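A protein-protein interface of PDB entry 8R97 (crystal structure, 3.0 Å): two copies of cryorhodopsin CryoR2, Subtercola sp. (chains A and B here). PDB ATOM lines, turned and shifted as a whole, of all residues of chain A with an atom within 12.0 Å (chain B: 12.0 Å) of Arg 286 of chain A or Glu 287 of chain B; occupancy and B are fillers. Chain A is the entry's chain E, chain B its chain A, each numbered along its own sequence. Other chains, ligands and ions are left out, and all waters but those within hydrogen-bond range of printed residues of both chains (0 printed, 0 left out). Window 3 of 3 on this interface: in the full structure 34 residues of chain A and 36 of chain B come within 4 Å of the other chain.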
ATOM      1  N   VAL A 261      -7.534  33.204  10.957  1.00  0.00           N
ATOM      2  CA  VAL A 261      -6.597  32.327  10.191  1.00  0.00           C
ATOM      3  C   VAL A 261      -5.163  32.639  10.630  1.00  0.00           C
ATOM      4  O   VAL A 261      -4.454  31.695  11.033  1.00  0.00           O
ATOM      5  CB  VAL A 261      -6.761  32.500   8.669  1.00  0.00           C
ATOM      6  CG1 VAL A 261      -5.652  31.795   7.900  1.00  0.00           C
ATOM      7  CG2 VAL A 261      -8.127  32.033   8.193  1.00  0.00           C
ATOM      8  N   GLY A 264      -4.200  31.727  13.993  1.00  0.00           N
ATOM      9  CA  GLY A 264      -4.149  30.252  14.066  1.00  0.00           C
ATOM     10  C   GLY A 264      -5.314  29.681  14.862  1.00  0.00           C
ATOM     11  O   GLY A 264      -5.185  28.552  15.378  1.00  0.00           O
ATOM     12  N   ASP A 265      -6.412  30.438  14.960  1.00  0.00           N
ATOM     13  CA  ASP A 265      -7.655  30.050  15.683  1.00  0.00           C
ATOM     14  C   ASP A 265      -8.478  29.100  14.806  1.00  0.00           C
ATOM     15  O   ASP A 265      -9.164  28.225  15.368  1.00  0.00           O
ATOM     16  CB  ASP A 265      -8.480  31.279  16.075  1.00  0.00           C
ATOM     17  CG  ASP A 265      -7.846  32.131  17.163  1.00  0.00           C
ATOM     18  OD1 ASP A 265      -6.885  31.656  17.800  1.00  0.00           O
ATOM     19  OD2 ASP A 265      -8.320  33.265  17.367  1.00  0.00           O
ATOM     20  N   ASP A 266      -8.411  29.271  13.482  1.00  0.00           N
ATOM     21  CA  ASP A 266      -9.158  28.454  12.488  1.00  0.00           C
ATOM     22  C   ASP A 266      -8.347  28.405  11.187  1.00  0.00           C
ATOM     23  O   ASP A 266      -7.218  28.933  11.177  1.00  0.00           O
ATOM     24  CB  ASP A 266     -10.565  29.021  12.278  1.00  0.00           C
ATOM     25  CG  ASP A 266     -11.580  28.007  11.776  1.00  0.00           C
ATOM     26  OD1 ASP A 266     -12.763  28.378  11.666  1.00  0.00           O
ATOM     27  OD2 ASP A 266     -11.181  26.853  11.508  1.00  0.00           O
ATOM     28  N   VAL A 267      -8.899  27.790  10.136  1.00  0.00           N
ATOM     29  CA  VAL A 267      -8.256  27.666   8.794  1.00  0.00           C
ATOM     30  C   VAL A 267      -9.318  27.915   7.715  1.00  0.00           C
ATOM     31  O   VAL A 267     -10.503  27.632   7.972  1.00  0.00           O
ATOM     32  CB  VAL A 267      -7.576  26.291   8.624  1.00  0.00           C
ATOM     33  CG1 VAL A 267      -8.553  25.146   8.840  1.00  0.00           C
ATOM     34  CG2 VAL A 267      -6.885  26.164   7.275  1.00  0.00           C
ATOM     35  N   HIS A 268      -8.903  28.442   6.561  1.00  0.00           N
ATOM     36  CA  HIS A 268      -9.778  28.741   5.395  1.00  0.00           C
ATOM     37  C   HIS A 268      -9.160  28.110   4.147  1.00  0.00           C
ATOM     38  O   HIS A 268      -7.954  28.208   3.934  1.00  0.00           O
ATOM     39  CB  HIS A 268      -9.998  30.256   5.282  1.00  0.00           C
ATOM     40  CG  HIS A 268     -11.276  30.625   4.610  1.00  0.00           C
ATOM     41  ND1 HIS A 268     -11.335  30.988   3.278  1.00  0.00           N
ATOM     42  CD2 HIS A 268     -12.540  30.682   5.079  1.00  0.00           C
ATOM     43  CE1 HIS A 268     -12.583  31.253   2.956  1.00  0.00           C
ATOM     44  NE2 HIS A 268     -13.342  31.074   4.043  1.00  0.00           N
ATOM     45  N   PRO A 269      -9.968  27.456   3.282  1.00  0.00           N
ATOM     46  CA  PRO A 269      -9.439  26.695   2.146  1.00  0.00           C
ATOM     47  C   PRO A 269      -8.947  27.525   0.949  1.00  0.00           C
ATOM     48  O   PRO A 269      -8.403  26.945   0.024  1.00  0.00           O
ATOM     49  CB  PRO A 269     -10.655  25.853   1.729  1.00  0.00           C
ATOM     50  CG  PRO A 269     -11.840  26.731   2.063  1.00  0.00           C
ATOM     51  CD  PRO A 269     -11.438  27.430   3.344  1.00  0.00           C
ATOM     52  N   GLU A 270      -9.146  28.844   0.985  1.00  0.00           N
ATOM     53  CA  GLU A 270      -8.730  29.778  -0.094  1.00  0.00           C
ATOM     54  C   GLU A 270      -8.119  31.030   0.536  1.00  0.00           C
ATOM     55  O   GLU A 270      -8.455  31.337   1.696  1.00  0.00           O
ATOM     56  CB  GLU A 270      -9.926  30.175  -0.961  1.00  0.00           C
ATOM     57  CG  GLU A 270     -10.872  31.149  -0.277  1.00  0.00           C
ATOM     58  CD  GLU A 270     -12.046  31.608  -1.127  1.00  0.00           C
ATOM     59  OE1 GLU A 270     -12.243  31.036  -2.219  1.00  0.00           O
ATOM     60  OE2 GLU A 270     -12.754  32.547  -0.705  1.00  0.00           O
ATOM     61  N   ASP A 281      -3.687  33.384   3.810  1.00  0.00           N
ATOM     62  CA  ASP A 281      -3.225  32.397   2.796  1.00  0.00           C
ATOM     63  C   ASP A 281      -4.120  31.159   2.906  1.00  0.00           C
ATOM     64  O   ASP A 281      -4.684  30.936   4.000  1.00  0.00           O
ATOM     65  CB  ASP A 281      -1.749  32.040   2.982  1.00  0.00           C
ATOM     66  CG  ASP A 281      -0.799  33.223   2.891  1.00  0.00           C
ATOM     67  OD1 ASP A 281       0.423  32.986   2.884  1.00  0.00           O
ATOM     68  OD2 ASP A 281      -1.288  34.371   2.843  1.00  0.00           O
ATOM     69  N   ALA A 282      -4.257  30.398   1.816  1.00  0.00           N
ATOM     70  CA  ALA A 282      -5.082  29.170   1.750  1.00  0.00           C
ATOM     71  C   ALA A 282      -4.495  28.115   2.694  1.00  0.00           C
ATOM     72  O   ALA A 282      -3.257  27.957   2.709  1.00  0.00           O
ATOM     73  CB  ALA A 282      -5.147  28.669   0.330  1.00  0.00           C
ATOM     74  N   GLY A 283      -5.356  27.436   3.458  1.00  0.00           N
ATOM     75  CA  GLY A 283      -4.976  26.385   4.422  1.00  0.00           C
ATOM     76  C   GLY A 283      -6.028  25.291   4.482  1.00  0.00           C
ATOM     77  O   GLY A 283      -7.225  25.619   4.373  1.00  0.00           O
ATOM     78  N   LEU A 284      -5.606  24.033   4.628  1.00  0.00           N
ATOM     79  CA  LEU A 284      -6.521  22.864   4.717  1.00  0.00           C
ATOM     80  C   LEU A 284      -6.503  22.318   6.138  1.00  0.00           C
ATOM     81  O   LEU A 284      -5.473  22.346   6.805  1.00  0.00           O
ATOM     82  CB  LEU A 284      -6.093  21.789   3.713  1.00  0.00           C
ATOM     83  CG  LEU A 284      -6.354  22.121   2.245  1.00  0.00           C
ATOM     84  CD1 LEU A 284      -5.970  20.952   1.349  1.00  0.00           C
ATOM     85  CD2 LEU A 284      -7.810  22.506   2.027  1.00  0.00           C
ATOM     86  N   PRO A 285      -7.658  21.839   6.649  1.00  0.00           N
ATOM     87  CA  PRO A 285      -7.710  21.191   7.958  1.00  0.00           C
ATOM     88  C   PRO A 285      -6.828  19.933   7.939  1.00  0.00           C
ATOM     89  O   PRO A 285      -6.667  19.357   6.879  1.00  0.00           O
ATOM     90  CB  PRO A 285      -9.194  20.841   8.152  1.00  0.00           C
ATOM     91  CG  PRO A 285      -9.934  21.716   7.151  1.00  0.00           C
ATOM     92  CD  PRO A 285      -8.973  21.910   5.996  1.00  0.00           C
ATOM     93  N   ARG A 286      -6.264  19.545   9.087  1.00  0.00           N
ATOM     94  CA  ARG A 286      -5.375  18.357   9.204  1.00  0.00           C
ATOM     95  C   ARG A 286      -6.218  17.084   9.078  1.00  0.00           C
ATOM     96  O   ARG A 286      -7.262  17.015   9.745  1.00  0.00           O
ATOM     97  CB  ARG A 286      -4.624  18.373  10.539  1.00  0.00           C
ATOM     98  N   GLU A 287      -5.792  16.127   8.247  1.00  0.00           N
ATOM     99  CA  GLU A 287      -6.469  14.809   8.088  1.00  0.00           C
ATOM    100  C   GLU A 287      -6.410  14.097   9.441  1.00  0.00           C
ATOM    101  O   GLU A 287      -5.320  14.070  10.036  1.00  0.00           O
ATOM    102  CB  GLU A 287      -5.812  13.976   6.987  1.00  0.00           C
ATOM    103  CG  GLU A 287      -6.003  14.554   5.596  1.00  0.00           C
ATOM    104  CD  GLU A 287      -5.229  13.851   4.494  1.00  0.00           C
ATOM    105  OE1 GLU A 287      -4.516  12.873   4.798  1.00  0.00           O
ATOM    106  OE2 GLU A 287      -5.340  14.290   3.334  1.00  0.00           O
ATOM    107  N   VAL A 288      -7.536  13.555   9.913  1.00  0.00           N
ATOM    108  CA  VAL A 288      -7.663  12.960  11.278  1.00  0.00           C
ATOM    109  C   VAL A 288      -8.053  11.481  11.165  1.00  0.00           C
ATOM    110  O   VAL A 288      -8.942  11.169  10.350  1.00  0.00           O
ATOM    111  CB  VAL A 288      -8.692  13.740  12.122  1.00  0.00           C
ATOM    112  CG1 VAL A 288      -8.823  13.170  13.524  1.00  0.00           C
ATOM    113  CG2 VAL A 288      -8.368  15.222  12.194  1.00  0.00           C
ATOM    114  N   TYR A 289      -7.407  10.618  11.961  1.00  0.00           N
ATOM    115  CA  TYR A 289      -7.737   9.178  12.140  1.00  0.00           C
ATOM    116  C   TYR A 289      -8.803   9.033  13.239  1.00  0.00           C
ATOM    117  O   TYR A 289      -8.747   9.786  14.232  1.00  0.00           O
ATOM    118  CB  TYR A 289      -6.497   8.379  12.545  1.00  0.00           C
ATOM    119  CG  TYR A 289      -5.501   8.114  11.446  1.00  0.00           C
ATOM    120  CD1 TYR A 289      -5.533   6.928  10.731  1.00  0.00           C
ATOM    121  CD2 TYR A 289      -4.510   9.030  11.138  1.00  0.00           C
ATOM    122  CE1 TYR A 289      -4.612   6.663   9.730  1.00  0.00           C
ATOM    123  CE2 TYR A 289      -3.583   8.783  10.138  1.00  0.00           C
ATOM    124  CZ  TYR A 289      -3.634   7.594   9.433  1.00  0.00           C
ATOM    125  OH  TYR A 289      -2.726   7.342   8.446  1.00  0.00           O
ATOM    126  N   LEU A 290      -9.729   8.082  13.081  1.00  0.00           N
ATOM    127  CA  LEU A 290     -10.853   7.859  14.033  1.00  0.00           C
ATOM    128  C   LEU A 290     -10.701   6.497  14.721  1.00  0.00           C
ATOM    129  O   LEU A 290     -10.932   6.380  15.930  1.00  0.00           O
ATOM    130  CB  LEU A 290     -12.174   7.958  13.265  1.00  0.00           C
ATOM    131  CG  LEU A 290     -12.427   9.298  12.574  1.00  0.00           C
ATOM    132  CD1 LEU A 290     -13.803   9.326  11.927  1.00  0.00           C
ATOM    133  CD2 LEU A 290     -12.274  10.454  13.554  1.00  0.00           C
ATOM    134  N   VAL B 267      -2.262  29.021  -4.741  1.00  0.00           N
ATOM    135  CA  VAL B 267      -2.549  27.651  -5.266  1.00  0.00           C
ATOM    136  C   VAL B 267      -4.017  27.597  -5.706  1.00  0.00           C
ATOM    137  O   VAL B 267      -4.833  28.345  -5.133  1.00  0.00           O
ATOM    138  CB  VAL B 267      -2.224  26.572  -4.214  1.00  0.00           C
ATOM    139  CG1 VAL B 267      -2.972  26.812  -2.916  1.00  0.00           C
ATOM    140  CG2 VAL B 267      -2.490  25.168  -4.731  1.00  0.00           C
ATOM    141  N   GLY B 283      -3.469  22.081  -7.515  1.00  0.00           N
ATOM    142  CA  GLY B 283      -2.699  22.121  -6.257  1.00  0.00           C
ATOM    143  C   GLY B 283      -3.604  22.350  -5.061  1.00  0.00           C
ATOM    144  O   GLY B 283      -4.593  23.097  -5.197  1.00  0.00           O
ATOM    145  N   LEU B 284      -3.282  21.721  -3.929  1.00  0.00           N
ATOM    146  CA  LEU B 284      -4.036  21.863  -2.657  1.00  0.00           C
ATOM    147  C   LEU B 284      -3.185  22.638  -1.660  1.00  0.00           C
ATOM    148  O   LEU B 284      -1.962  22.516  -1.651  1.00  0.00           O
ATOM    149  CB  LEU B 284      -4.394  20.477  -2.108  1.00  0.00           C
ATOM    150  CG  LEU B 284      -5.484  19.734  -2.875  1.00  0.00           C
ATOM    151  CD1 LEU B 284      -5.813  18.409  -2.203  1.00  0.00           C
ATOM    152  CD2 LEU B 284      -6.731  20.598  -3.008  1.00  0.00           C
ATOM    153  N   PRO B 285      -3.813  23.480  -0.811  1.00  0.00           N
ATOM    154  CA  PRO B 285      -3.089  24.185   0.243  1.00  0.00           C
ATOM    155  C   PRO B 285      -2.491  23.166   1.223  1.00  0.00           C
ATOM    156  O   PRO B 285      -3.024  22.075   1.323  1.00  0.00           O
ATOM    157  CB  PRO B 285      -4.154  25.060   0.923  1.00  0.00           C
ATOM    158  CG  PRO B 285      -5.301  25.122  -0.073  1.00  0.00           C
ATOM    159  CD  PRO B 285      -5.242  23.819  -0.842  1.00  0.00           C
ATOM    160  N   ARG B 286      -1.406  23.537   1.907  1.00  0.00           N
ATOM    161  CA  ARG B 286      -0.735  22.694   2.935  1.00  0.00           C
ATOM    162  C   ARG B 286      -1.657  22.537   4.152  1.00  0.00           C
ATOM    163  O   ARG B 286      -2.214  23.561   4.605  1.00  0.00           O
ATOM    164  CB  ARG B 286       0.596  23.326   3.354  1.00  0.00           C
ATOM    165  CG  ARG B 286       0.498  24.794   3.744  1.00  0.00           C
ATOM    166  CD  ARG B 286       0.468  25.005   5.249  1.00  0.00           C
ATOM    167  N   GLU B 287      -1.817  21.304   4.649  1.00  0.00           N
ATOM    168  CA  GLU B 287      -2.633  20.983   5.852  1.00  0.00           C
ATOM    169  C   GLU B 287      -2.069  21.763   7.042  1.00  0.00           C
ATOM    170  O   GLU B 287      -0.836  21.738   7.230  1.00  0.00           O
ATOM    171  CB  GLU B 287      -2.622  19.481   6.147  1.00  0.00           C
ATOM    172  CG  GLU B 287      -3.406  18.650   5.150  1.00  0.00           C
ATOM    173  CD  GLU B 287      -3.502  17.177   5.512  1.00  0.00           C
ATOM    174  OE1 GLU B 287      -3.264  16.845   6.691  1.00  0.00           O
ATOM    175  OE2 GLU B 287      -3.809  16.367   4.614  1.00  0.00           O
ATOM    176  N   VAL B 288      -2.937  22.420   7.816  1.00  0.00           N
ATOM    177  CA  VAL B 288      -2.526  23.296   8.952  1.00  0.00           C
ATOM    178  C   VAL B 288      -3.071  22.734  10.269  1.00  0.00           C
ATOM    179  O   VAL B 288      -4.266  22.388  10.324  1.00  0.00           O
ATOM    180  CB  VAL B 288      -2.988  24.748   8.730  1.00  0.00           C
ATOM    181  CG1 VAL B 288      -2.544  25.655   9.866  1.00  0.00           C
ATOM    182  CG2 VAL B 288      -2.509  25.296   7.394  1.00  0.00           C
ATOM    183  N   TYR B 289      -2.197  22.636  11.274  1.00  0.00           N
ATOM    184  CA  TYR B 289      -2.514  22.237  12.671  1.00  0.00           C
ATOM    185  C   TYR B 289      -2.774  23.531  13.457  1.00  0.00           C
ATOM    186  O   TYR B 289      -2.016  24.500  13.253  1.00  0.00           O
ATOM    187  CB  TYR B 289      -1.363  21.434  13.288  1.00  0.00           C
ATOM    188  CG  TYR B 289      -0.713  20.415  12.382  1.00  0.00           C
ATOM    189  CD1 TYR B 289      -1.128  19.093  12.372  1.00  0.00           C
ATOM    190  CD2 TYR B 289       0.331  20.769  11.543  1.00  0.00           C
ATOM    191  CE1 TYR B 289      -0.529  18.154  11.548  1.00  0.00           C
ATOM    192  CE2 TYR B 289       0.940  19.843  10.712  1.00  0.00           C
ATOM    193  CZ  TYR B 289       0.507  18.530  10.715  1.00  0.00           C
ATOM    194  OH  TYR B 289       1.098  17.606   9.902  1.00  0.00           O
ATOM    195  N   LEU B 290      -3.803  23.562  14.310  1.00  0.00           N
ATOM    196  CA  LEU B 290      -4.207  24.785  15.060  1.00  0.00           C
ATOM    197  C   LEU B 290      -3.955  24.604  16.563  1.00  0.00           C
ATOM    198  O   LEU B 290      -3.543  23.551  17.045  1.00  0.00           O
ATOM    199  CB  LEU B 290      -5.685  25.071  14.777  1.00  0.00           C
ATOM    200  CG  LEU B 290      -6.068  25.165  13.300  1.00  0.00           C
ATOM    201  CD1 LEU B 290      -7.568  25.365  13.138  1.00  0.00           C
ATOM    202  CD2 LEU B 290      -5.306  26.283  12.608  1.00  0.00           C
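O of Arg 286 of chain B is in hydrogen-bond range of N of Leu 284 of chain A, 3.4 Å away.
The side-chain carboxylate of Glu 287 of chain B is in hydrogen-bond range of the backbone NH of Glu 287 of chain A (3.1 Å).
The backbone NH (N) of Val 288 of chain B sits at hydrogen-bond distance from the backbone carbonyl oxygen (O) of Leu 284 of chain A (2.7 Å).
The backbone carbonyl oxygen (O) of His 268 of chain A is in hydrogen-bond range of the backbone NH (N) of Gly 283 of chain A, at 2.8 Å.
Leu 290 of chain B touches Asp 265 of chain A (CD1 to O, 3.96 Å).
CA of Asp 266 of chain A touches CD1 of Leu 290 of chain B, 3.5 Å away.
Pro 269 of chain A touches Pro 285 of chain B (O to CG, 3.6 Å).
CB of Pro 285 of chain B touches O of Ala 282 of chain A (3.5 Å).
O of Arg 286 of chain B touches CA of Gly 283 of chain A (3.95 Å).
Leu 284 of chain A touches Pro 285 of chain B (CD1 to O, 3.2 Å).
O of Leu 284 of chain A touches CA of Glu 287 of chain B (3.3 Å).
Glu 287 of chain B touches Pro 285 of chain A.
Arg 286 of chain A touches Glu 287 of chain B (CA to OE1, 3.6 Å).
N of Arg 286 of chain A touches O of Val 288 of chain B, 3.7 Å away.
Of the printed residues of chain A, Glu 287 of chain B touches Leu 284 (3.3 Å), Pro 285 (3.8 Å), Arg 286 (3.6 Å) and Glu 287 (2.9 Å).
Of the printed residues of chain B, Leu 284 of chain A touches Leu 284, Pro 285, Arg 286, Glu 287 and Val 288.
Pro 285 of chain A touches just one residue of chain B: Glu 287.
Glu 287 of chain A touches just one residue of chain B: Glu 287 (2.9 Å).
No residue of chain B comes within 4 Å of Val 288 of chain A.
Pro 285 of chain B touches four residues of chain A.
Arg 286 of chain B touches two residues of chain A.
Of the printed residues of chain B, Asp 266 of chain A touches Leu 290.
Printed residues of chain B within 4 Å of Ala 282 of chain A: Pro 285.
Of the printed residues of chain B, Asp 265 of chain A touches Leu 290.
Printed residues of chain A within 4 Å of Leu 284 of chain B: Leu 284.
Of the printed residues of chain B, Gly 264 of chain A touches Leu 290 (3.6 Å).
The nearest printed residue of chain B that does not touch Arg 286 of chain A is Tyr 289 of chain B (4.01 Å).
The nearest residue of chain A that does not touch Glu 287 of chain B is Gly 283 of chain A (5.7 Å).
The nearest printed residue of chain B that does not touch Ala 282 of chain A is Val 267 of chain B (4.3 Å).
Of the 9 printed residues of chain B, 6 touch a printed residue of chain A.
Hydrophobic or aromatic side chains of chain B that line the printed part of chain A: Leu 284, Pro 285, Val 288 and Leu 290.
Of the 18 printed residues of chain A, 10 touch a printed residue of chain B.
Printed residues of chain A that touch a printed residue of chain B: Gly 264, Asp 265, Asp 266, Pro 269, Ala 282, Gly 283, Leu 284, Pro 285, Arg 286 and Glu 287.
Hydrophobic or aromatic side chains of chain A that line the printed part of chain B: Ala 282 and Leu 284.
Among the printed residues, 16 pairs touch across the chains.
Among the printed residues, no Asp or Glu carboxylate lies within 4 Å of a Lys or Arg side-chain nitrogen of the other chain.
Gly 283 of chain A touches Pro 285 of chain B, but with the chains exchanged Pro 285 of chain A does not touch Gly 283 of chain B (12.1 Å).
Leu 284 of chain A touches Pro 285 of chain B, but with the chains exchanged Pro 285 of chain A does not touch Leu 284 of chain B (9.2 Å).
Arg 286 of chain A touches Val 288 of chain B, but with the chains exchanged Val 288 of chain A does not touch Arg 286 of chain B (12.2 Å).
Glu 287 of chain B touches its own counterpart, Glu 287 of chain A.
Positions printed for both chains: 267, 283, 284, 285, 286, 287, 288, 289 and 290.
Of the 16 pairs that touch across the chains among the printed residues, 2 have their exchanged pair printed and touching as well.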
